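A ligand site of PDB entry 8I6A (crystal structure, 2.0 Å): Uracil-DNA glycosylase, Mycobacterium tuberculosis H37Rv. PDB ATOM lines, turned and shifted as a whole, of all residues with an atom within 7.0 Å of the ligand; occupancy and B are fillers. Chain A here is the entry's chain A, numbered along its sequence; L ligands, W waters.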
ATOM      1  N   VAL A  76      26.646  11.083  -1.231  1.00  0.00           N
ATOM      2  CA  VAL A  76      27.948  11.772  -1.031  1.00  0.00           C
ATOM      3  C   VAL A  76      28.240  12.672  -2.226  1.00  0.00           C
ATOM      4  O   VAL A  76      28.358  12.131  -3.331  1.00  0.00           O
ATOM      5  CB  VAL A  76      29.099  10.784  -0.869  1.00  0.00           C
ATOM      6  CG1 VAL A  76      30.369  11.553  -0.510  1.00  0.00           C
ATOM      7  CG2 VAL A  76      28.788   9.703   0.151  1.00  0.00           C
ATOM      8  N   GLY A  77      28.448  13.970  -1.975  1.00  0.00           N
ATOM      9  CA  GLY A  77      29.049  14.923  -2.922  1.00  0.00           C
ATOM     10  C   GLY A  77      30.486  15.261  -2.545  1.00  0.00           C
ATOM     11  O   GLY A  77      31.028  14.669  -1.546  1.00  0.00           O
ATOM     12  N   GLN A  78      31.116  16.183  -3.275  1.00  0.00           N
ATOM     13  CA  GLN A  78      32.541  16.500  -3.051  1.00  0.00           C
ATOM     14  C   GLN A  78      32.603  17.884  -2.398  1.00  0.00           C
ATOM     15  O   GLN A  78      32.935  17.942  -1.217  1.00  0.00           O
ATOM     16  CB  GLN A  78      33.363  16.297  -4.322  1.00  0.00           C
ATOM     17  CG  GLN A  78      34.885  16.511  -4.141  1.00  0.00           C
ATOM     18  CD  GLN A  78      35.504  15.898  -2.906  1.00  0.00           C
ATOM     19  OE1 GLN A  78      36.098  16.598  -2.078  1.00  0.00           O
ATOM     20  NE2 GLN A  78      35.364  14.586  -2.739  1.00  0.00           N
ATOM     21  N   ASP A  79      32.213  18.947  -3.106  1.00  0.00           N
ATOM     22  CA  ASP A  79      32.333  20.339  -2.575  1.00  0.00           C
ATOM     23  C   ASP A  79      31.001  21.054  -2.721  1.00  0.00           C
ATOM     24  O   ASP A  79      30.263  20.726  -3.649  1.00  0.00           O
ATOM     25  CB  ASP A  79      33.377  21.137  -3.341  1.00  0.00           C
ATOM     26  CG  ASP A  79      34.781  20.581  -3.244  1.00  0.00           C
ATOM     27  OD1 ASP A  79      35.422  20.781  -2.201  1.00  0.00           O
ATOM     28  OD2 ASP A  79      35.227  20.011  -4.242  1.00  0.00           O
ATOM     29  N   PRO A  80      30.703  22.074  -1.888  1.00  0.00           N
ATOM     30  CA  PRO A  80      29.496  22.858  -2.083  1.00  0.00           C
ATOM     31  C   PRO A  80      29.533  23.556  -3.447  1.00  0.00           C
ATOM     32  O   PRO A  80      30.623  23.758  -4.012  1.00  0.00           O
ATOM     33  CB  PRO A  80      29.496  23.843  -0.895  1.00  0.00           C
ATOM     34  CG  PRO A  80      30.514  23.259   0.071  1.00  0.00           C
ATOM     35  CD  PRO A  80      31.540  22.631  -0.824  1.00  0.00           C
ATOM     36  N   TYR A  81      28.373  23.964  -3.943  1.00  0.00           N
ATOM     37  CA  TYR A  81      28.275  24.862  -5.119  1.00  0.00           C
ATOM     38  C   TYR A  81      29.189  26.071  -4.881  1.00  0.00           C
ATOM     39  O   TYR A  81      29.146  26.685  -3.810  1.00  0.00           O
ATOM     40  CB  TYR A  81      26.840  25.365  -5.354  1.00  0.00           C
ATOM     41  CG  TYR A  81      25.869  24.318  -5.799  1.00  0.00           C
ATOM     42  CD1 TYR A  81      25.989  23.711  -7.040  1.00  0.00           C
ATOM     43  CD2 TYR A  81      24.811  23.925  -4.981  1.00  0.00           C
ATOM     44  CE1 TYR A  81      25.085  22.760  -7.479  1.00  0.00           C
ATOM     45  CE2 TYR A  81      23.904  22.957  -5.402  1.00  0.00           C
ATOM     46  CZ  TYR A  81      24.035  22.371  -6.650  1.00  0.00           C
ATOM     47  OH  TYR A  81      23.126  21.436  -7.065  1.00  0.00           O
ATOM     48  N   PRO A  82      30.003  26.444  -5.887  1.00  0.00           N
ATOM     49  CA  PRO A  82      30.847  27.631  -5.799  1.00  0.00           C
ATOM     50  C   PRO A  82      30.165  28.974  -6.113  1.00  0.00           C
ATOM     51  O   PRO A  82      30.676  30.038  -5.754  1.00  0.00           O
ATOM     52  CB  PRO A  82      31.942  27.330  -6.837  1.00  0.00           C
ATOM     53  CG  PRO A  82      31.286  26.403  -7.880  1.00  0.00           C
ATOM     54  CD  PRO A  82      30.177  25.688  -7.149  1.00  0.00           C
ATOM     55  N   ALA A  87      24.826  27.271  -2.527  1.00  0.00           N
ATOM     56  CA  ALA A  87      25.139  26.315  -1.425  1.00  0.00           C
ATOM     57  C   ALA A  87      24.266  26.602  -0.207  1.00  0.00           C
ATOM     58  O   ALA A  87      24.235  27.760   0.259  1.00  0.00           O
ATOM     59  CB  ALA A  87      26.585  26.387  -1.072  1.00  0.00           C
ATOM     60  N   LEU A  90      23.206  21.295   2.358  1.00  0.00           N
ATOM     61  CA  LEU A  90      22.796  19.941   1.942  1.00  0.00           C
ATOM     62  C   LEU A  90      23.321  19.746   0.524  1.00  0.00           C
ATOM     63  O   LEU A  90      23.067  20.615  -0.331  1.00  0.00           O
ATOM     64  CB  LEU A  90      21.266  19.836   1.971  1.00  0.00           C
ATOM     65  CG  LEU A  90      20.568  20.102   3.314  1.00  0.00           C
ATOM     66  CD1 LEU A  90      19.066  19.928   3.156  1.00  0.00           C
ATOM     67  CD2 LEU A  90      21.092  19.181   4.404  1.00  0.00           C
ATOM     68  N   SER A  91      24.025  18.668   0.277  1.00  0.00           N
ATOM     69  CA  SER A  91      24.675  18.433  -1.038  1.00  0.00           C
ATOM     70  C   SER A  91      23.601  18.517  -2.123  1.00  0.00           C
ATOM     71  O   SER A  91      22.478  17.963  -1.904  1.00  0.00           O
ATOM     72  CB  SER A  91      25.423  17.138  -1.065  1.00  0.00           C
ATOM     73  OG  SER A  91      24.555  16.050  -0.926  1.00  0.00           O
ATOM     74  N   PHE A  92      23.925  19.274  -3.200  1.00  0.00           N
ATOM     75  CA  PHE A  92      23.123  19.457  -4.452  1.00  0.00           C
ATOM     76  C   PHE A  92      21.862  20.308  -4.262  1.00  0.00           C
ATOM     77  O   PHE A  92      21.301  20.760  -5.290  1.00  0.00           O
ATOM     78  CB  PHE A  92      22.795  18.099  -5.047  1.00  0.00           C
ATOM     79  CG  PHE A  92      24.019  17.266  -5.345  1.00  0.00           C
ATOM     80  CD1 PHE A  92      24.838  17.554  -6.436  1.00  0.00           C
ATOM     81  CD2 PHE A  92      24.352  16.201  -4.535  1.00  0.00           C
ATOM     82  CE1 PHE A  92      25.970  16.786  -6.691  1.00  0.00           C
ATOM     83  CE2 PHE A  92      25.496  15.441  -4.792  1.00  0.00           C
ATOM     84  CZ  PHE A  92      26.308  15.758  -5.863  1.00  0.00           C
ATOM     85  N   SER A  93      21.419  20.568  -3.024  1.00  0.00           N
ATOM     86  CA  SER A  93      20.195  21.361  -2.772  1.00  0.00           C
ATOM     87  C   SER A  93      20.439  22.839  -3.112  1.00  0.00           C
ATOM     88  O   SER A  93      21.572  23.349  -2.924  1.00  0.00           O
ATOM     89  CB  SER A  93      19.710  21.195  -1.334  1.00  0.00           C
ATOM     90  OG  SER A  93      18.362  21.601  -1.193  1.00  0.00           O
ATOM     91  N   PRO A 102      21.093  24.637 -10.888  1.00  0.00           N
ATOM     92  CA  PRO A 102      22.433  24.227 -11.300  1.00  0.00           C
ATOM     93  C   PRO A 102      22.337  22.945 -12.142  1.00  0.00           C
ATOM     94  O   PRO A 102      21.422  22.127 -11.946  1.00  0.00           O
ATOM     95  CB  PRO A 102      23.178  23.989  -9.987  1.00  0.00           C
ATOM     96  CG  PRO A 102      22.403  24.777  -8.956  1.00  0.00           C
ATOM     97  CD  PRO A 102      20.977  24.826  -9.453  1.00  0.00           C
ATOM     98  N   ARG A 103      23.324  22.767 -13.022  1.00  0.00           N
ATOM     99  CA  ARG A 103      23.347  21.680 -14.041  1.00  0.00           C
ATOM    100  C   ARG A 103      23.253  20.334 -13.308  1.00  0.00           C
ATOM    101  O   ARG A 103      22.478  19.489 -13.742  1.00  0.00           O
ATOM    102  CB  ARG A 103      24.618  21.812 -14.895  1.00  0.00           C
ATOM    103  N   SER A 104      24.003  20.134 -12.238  1.00  0.00           N
ATOM    104  CA  SER A 104      24.025  18.831 -11.502  1.00  0.00           C
ATOM    105  C   SER A 104      22.602  18.514 -11.046  1.00  0.00           C
ATOM    106  O   SER A 104      22.136  17.369 -11.223  1.00  0.00           O
ATOM    107  CB  SER A 104      24.979  18.851 -10.352  1.00  0.00           C
ATOM    108  OG  SER A 104      26.303  18.688 -10.809  1.00  0.00           O
ATOM    109  N   LEU A 105      21.923  19.518 -10.516  1.00  0.00           N
ATOM    110  CA  LEU A 105      20.579  19.343  -9.910  1.00  0.00           C
ATOM    111  C   LEU A 105      19.551  19.089 -11.013  1.00  0.00           C
ATOM    112  O   LEU A 105      18.695  18.219 -10.800  1.00  0.00           O
ATOM    113  CB  LEU A 105      20.220  20.556  -9.041  1.00  0.00           C
ATOM    114  CG  LEU A 105      18.902  20.396  -8.279  1.00  0.00           C
ATOM    115  CD1 LEU A 105      18.995  19.191  -7.352  1.00  0.00           C
ATOM    116  CD2 LEU A 105      18.511  21.671  -7.522  1.00  0.00           C
ATOM    117  N   LEU A 136      22.514  14.261   2.894  1.00  0.00           N
ATOM    118  CA  LEU A 136      23.057  14.929   1.698  1.00  0.00           C
ATOM    119  C   LEU A 136      24.396  15.531   2.106  1.00  0.00           C
ATOM    120  O   LEU A 136      24.447  16.733   2.419  1.00  0.00           O
ATOM    121  CB  LEU A 136      22.036  15.964   1.224  1.00  0.00           C
ATOM    122  CG  LEU A 136      20.749  15.380   0.640  1.00  0.00           C
ATOM    123  CD1 LEU A 136      19.644  16.451   0.611  1.00  0.00           C
ATOM    124  CD2 LEU A 136      20.958  14.835  -0.748  1.00  0.00           C
ATOM    125  N   LEU A 137      25.422  14.683   2.133  1.00  0.00           N
ATOM    126  CA  LEU A 137      26.762  14.995   2.693  1.00  0.00           C
ATOM    127  C   LEU A 137      27.793  15.278   1.605  1.00  0.00           C
ATOM    128  O   LEU A 137      28.135  14.373   0.812  1.00  0.00           O
ATOM    129  CB  LEU A 137      27.190  13.839   3.592  1.00  0.00           C
ATOM    130  CG  LEU A 137      28.494  14.047   4.361  1.00  0.00           C
ATOM    131  CD1 LEU A 137      28.389  15.239   5.267  1.00  0.00           C
ATOM    132  CD2 LEU A 137      28.861  12.820   5.179  1.00  0.00           C
ATOM    133  N   ASN A 138      28.357  16.490   1.609  1.00  0.00           N
ATOM    134  CA  ASN A 138      29.570  16.849   0.845  1.00  0.00           C
ATOM    135  C   ASN A 138      30.781  16.424   1.690  1.00  0.00           C
ATOM    136  O   ASN A 138      30.735  16.609   2.928  1.00  0.00           O
ATOM    137  CB  ASN A 138      29.569  18.339   0.485  1.00  0.00           C
ATOM    138  CG  ASN A 138      28.728  18.681  -0.724  1.00  0.00           C
ATOM    139  OD1 ASN A 138      28.693  17.877  -1.649  1.00  0.00           O
ATOM    140  ND2 ASN A 138      28.018  19.817  -0.703  1.00  0.00           N
ATOM    141  N   ARG A 139      31.837  15.908   1.089  1.00  0.00           N
ATOM    142  CA  ARG A 139      33.078  15.528   1.833  1.00  0.00           C
ATOM    143  C   ARG A 139      33.748  16.790   2.418  1.00  0.00           C
ATOM    144  O   ARG A 139      34.393  16.701   3.477  1.00  0.00           O
ATOM    145  CB  ARG A 139      34.050  14.793   0.919  1.00  0.00           C
ATOM    146  CG  ARG A 139      33.642  13.393   0.502  1.00  0.00           C
ATOM    147  CD  ARG A 139      33.466  12.347   1.598  1.00  0.00           C
ATOM    148  NE  ARG A 139      34.305  12.560   2.773  1.00  0.00           N
ATOM    149  CZ  ARG A 139      35.622  12.317   2.846  1.00  0.00           C
ATOM    150  NH1 ARG A 139      36.253  12.558   3.978  1.00  0.00           N
ATOM    151  NH2 ARG A 139      36.274  11.813   1.819  1.00  0.00           N
ATOM    152  N   TRP A 179      27.965  10.293  -5.517  1.00  0.00           N
ATOM    153  CA  TRP A 179      27.827  11.274  -6.628  1.00  0.00           C
ATOM    154  C   TRP A 179      28.999  12.243  -6.635  1.00  0.00           C
ATOM    155  O   TRP A 179      28.907  13.245  -7.337  1.00  0.00           O
ATOM    156  CB  TRP A 179      26.517  12.042  -6.534  1.00  0.00           C
ATOM    157  CG  TRP A 179      25.348  11.226  -6.967  1.00  0.00           C
ATOM    158  CD1 TRP A 179      25.349  10.024  -7.629  1.00  0.00           C
ATOM    159  CD2 TRP A 179      23.988  11.564  -6.745  1.00  0.00           C
ATOM    160  NE1 TRP A 179      24.065   9.603  -7.841  1.00  0.00           N
ATOM    161  CE2 TRP A 179      23.206  10.518  -7.308  1.00  0.00           C
ATOM    162  CE3 TRP A 179      23.350  12.668  -6.194  1.00  0.00           C
ATOM    163  CZ2 TRP A 179      21.812  10.544  -7.287  1.00  0.00           C
ATOM    164  CZ3 TRP A 179      21.985  12.678  -6.159  1.00  0.00           C
ATOM    165  CH2 TRP A 179      21.226  11.632  -6.683  1.00  0.00           C
ATOM    166  N   GLY A 180      30.081  11.942  -5.906  1.00  0.00           N
ATOM    167  CA  GLY A 180      31.329  12.720  -5.905  1.00  0.00           C
ATOM    168  C   GLY A 180      32.553  11.913  -6.312  1.00  0.00           C
ATOM    169  O   GLY A 180      33.654  12.289  -5.897  1.00  0.00           O
ATOM    170  N   PRO A 205      26.201  13.116 -11.373  1.00  0.00           N
ATOM    171  CA  PRO A 205      25.159  13.760 -12.159  1.00  0.00           C
ATOM    172  C   PRO A 205      25.662  14.424 -13.461  1.00  0.00           C
ATOM    173  O   PRO A 205      24.943  14.440 -14.423  1.00  0.00           O
ATOM    174  CB  PRO A 205      24.549  14.791 -11.203  1.00  0.00           C
ATOM    175  CG  PRO A 205      24.869  14.279  -9.828  1.00  0.00           C
ATOM    176  CD  PRO A 205      26.141  13.481  -9.957  1.00  0.00           C
ATOM    177  N   LEU A 206      26.922  14.898 -13.506  1.00  0.00           N
ATOM    178  CA  LEU A 206      27.471  15.549 -14.726  1.00  0.00           C
ATOM    179  C   LEU A 206      27.915  14.504 -15.781  1.00  0.00           C
ATOM    180  O   LEU A 206      28.126  14.887 -16.954  1.00  0.00           O
ATOM    181  CB  LEU A 206      28.571  16.519 -14.299  1.00  0.00           C
ATOM    182  CG  LEU A 206      28.079  17.698 -13.445  1.00  0.00           C
ATOM    183  CD1 LEU A 206      29.231  18.606 -13.029  1.00  0.00           C
ATOM    184  CD2 LEU A 206      27.026  18.498 -14.179  1.00  0.00           C
HETATM  185  N1  LIG L   1      28.721  18.991  -6.437  1.00  0.00           N
HETATM  186  C1  LIG L   1      28.799  18.284  -5.272  1.00  0.00           C
HETATM  187  O1  LIG L   1      29.535  17.306  -5.159  1.00  0.00           O
HETATM  188  N2  LIG L   1      28.034  18.754  -4.245  1.00  0.00           N
HETATM  189  C2  LIG L   1      27.237  19.876  -4.249  1.00  0.00           C
HETATM  190  O2  LIG L   1      26.623  20.208  -3.222  1.00  0.00           O
HETATM  191  C3  LIG L   1      27.210  20.588  -5.487  1.00  0.00           C
HETATM  192  C4  LIG L   1      27.972  20.130  -6.543  1.00  0.00           C
HETATM  193  C5  LIG L   1      28.003  20.831  -7.878  1.00  0.00           C
HETATM  194  O3  LIG L   1      28.784  21.817  -7.954  1.00  0.00           O
HETATM  195  O4  LIG L   1      27.231  20.415  -8.737  1.00  0.00           O
HETATM  196  O   HOH W   1      26.343  21.828 -11.129  1.00  0.00           O
HETATM  197  O   HOH W   2      30.732  21.556  -6.133  1.00  0.00           O
HETATM  198  O   HOH W   3      26.227  22.711  -2.036  1.00  0.00           O
HETATM  199  O   HOH W   4      32.219  19.244  -5.909  1.00  0.00           O
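The backbone carbonyl oxygen of Asp 79 sits at hydrogen-bond distance from a nitrogen (N2) of the ligand (3.0 Å).
The side-chain amide oxygen (OD1) of Asn 138 is in hydrogen-bond range of a nitrogen (N2) of the ligand (2.8 Å).
OG of Ser 104 lies within hydrogen-bond range of O4 of the ligand, 2.9 Å away.
The backbone NH of Gln 78 sits at hydrogen-bond distance from an oxygen (O1) of the ligand (2.7 Å).
N of Phe 92 sits at hydrogen-bond distance from O2 of the ligand, 2.9 Å away.
The side-chain amide oxygen of Asn 138 sits at hydrogen-bond distance from the backbone NH of Gln 78, 3.4 Å away.
The backbone carbonyl oxygen (O) of Phe 92 lies within hydrogen-bond range of the side-chain hydroxyl (OH) of Tyr 81, at 2.6 Å.
N of Arg 139 is in hydrogen-bond range of O of Gln 78, 3.3 Å away.
The backbone NH of Ser 91 sits at hydrogen-bond distance from the backbone carbonyl oxygen of Leu 136 (2.9 Å).
The backbone NH of Gly 77 is in hydrogen-bond range of the backbone carbonyl oxygen of Leu 137.
O of Gly 77 is in hydrogen-bond range of N of Arg 139 (3.0 Å).
OG of Ser 91 sits at hydrogen-bond distance from N of Leu 137, 3.5 Å away.
Residues that only touch the ligand: Gly 77 (3.3 Å), Tyr 81 (3.4 Å) and Ser 91 (3.4 Å).
Of the 24 residues printed, 8 come within 4 Å of the ligand.
Water W2 lies within hydrogen-bond range of O of Asp 79 (2.7 Å), O3 of the ligand (2.7 Å) and O of Pro 80 (3.1 Å).
Water W3 bridges O2 of the ligand (2.8 Å) and N of Tyr 81 (3.1 Å).
Water W1 lies within hydrogen-bond range of O4 of the ligand (2.9 Å) and N of Ser 104 (3.1 Å).
Water W4 bridges the backbone NH of Asp 79 (2.8 Å) and an oxygen (O1) of the ligand (3.4 Å).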
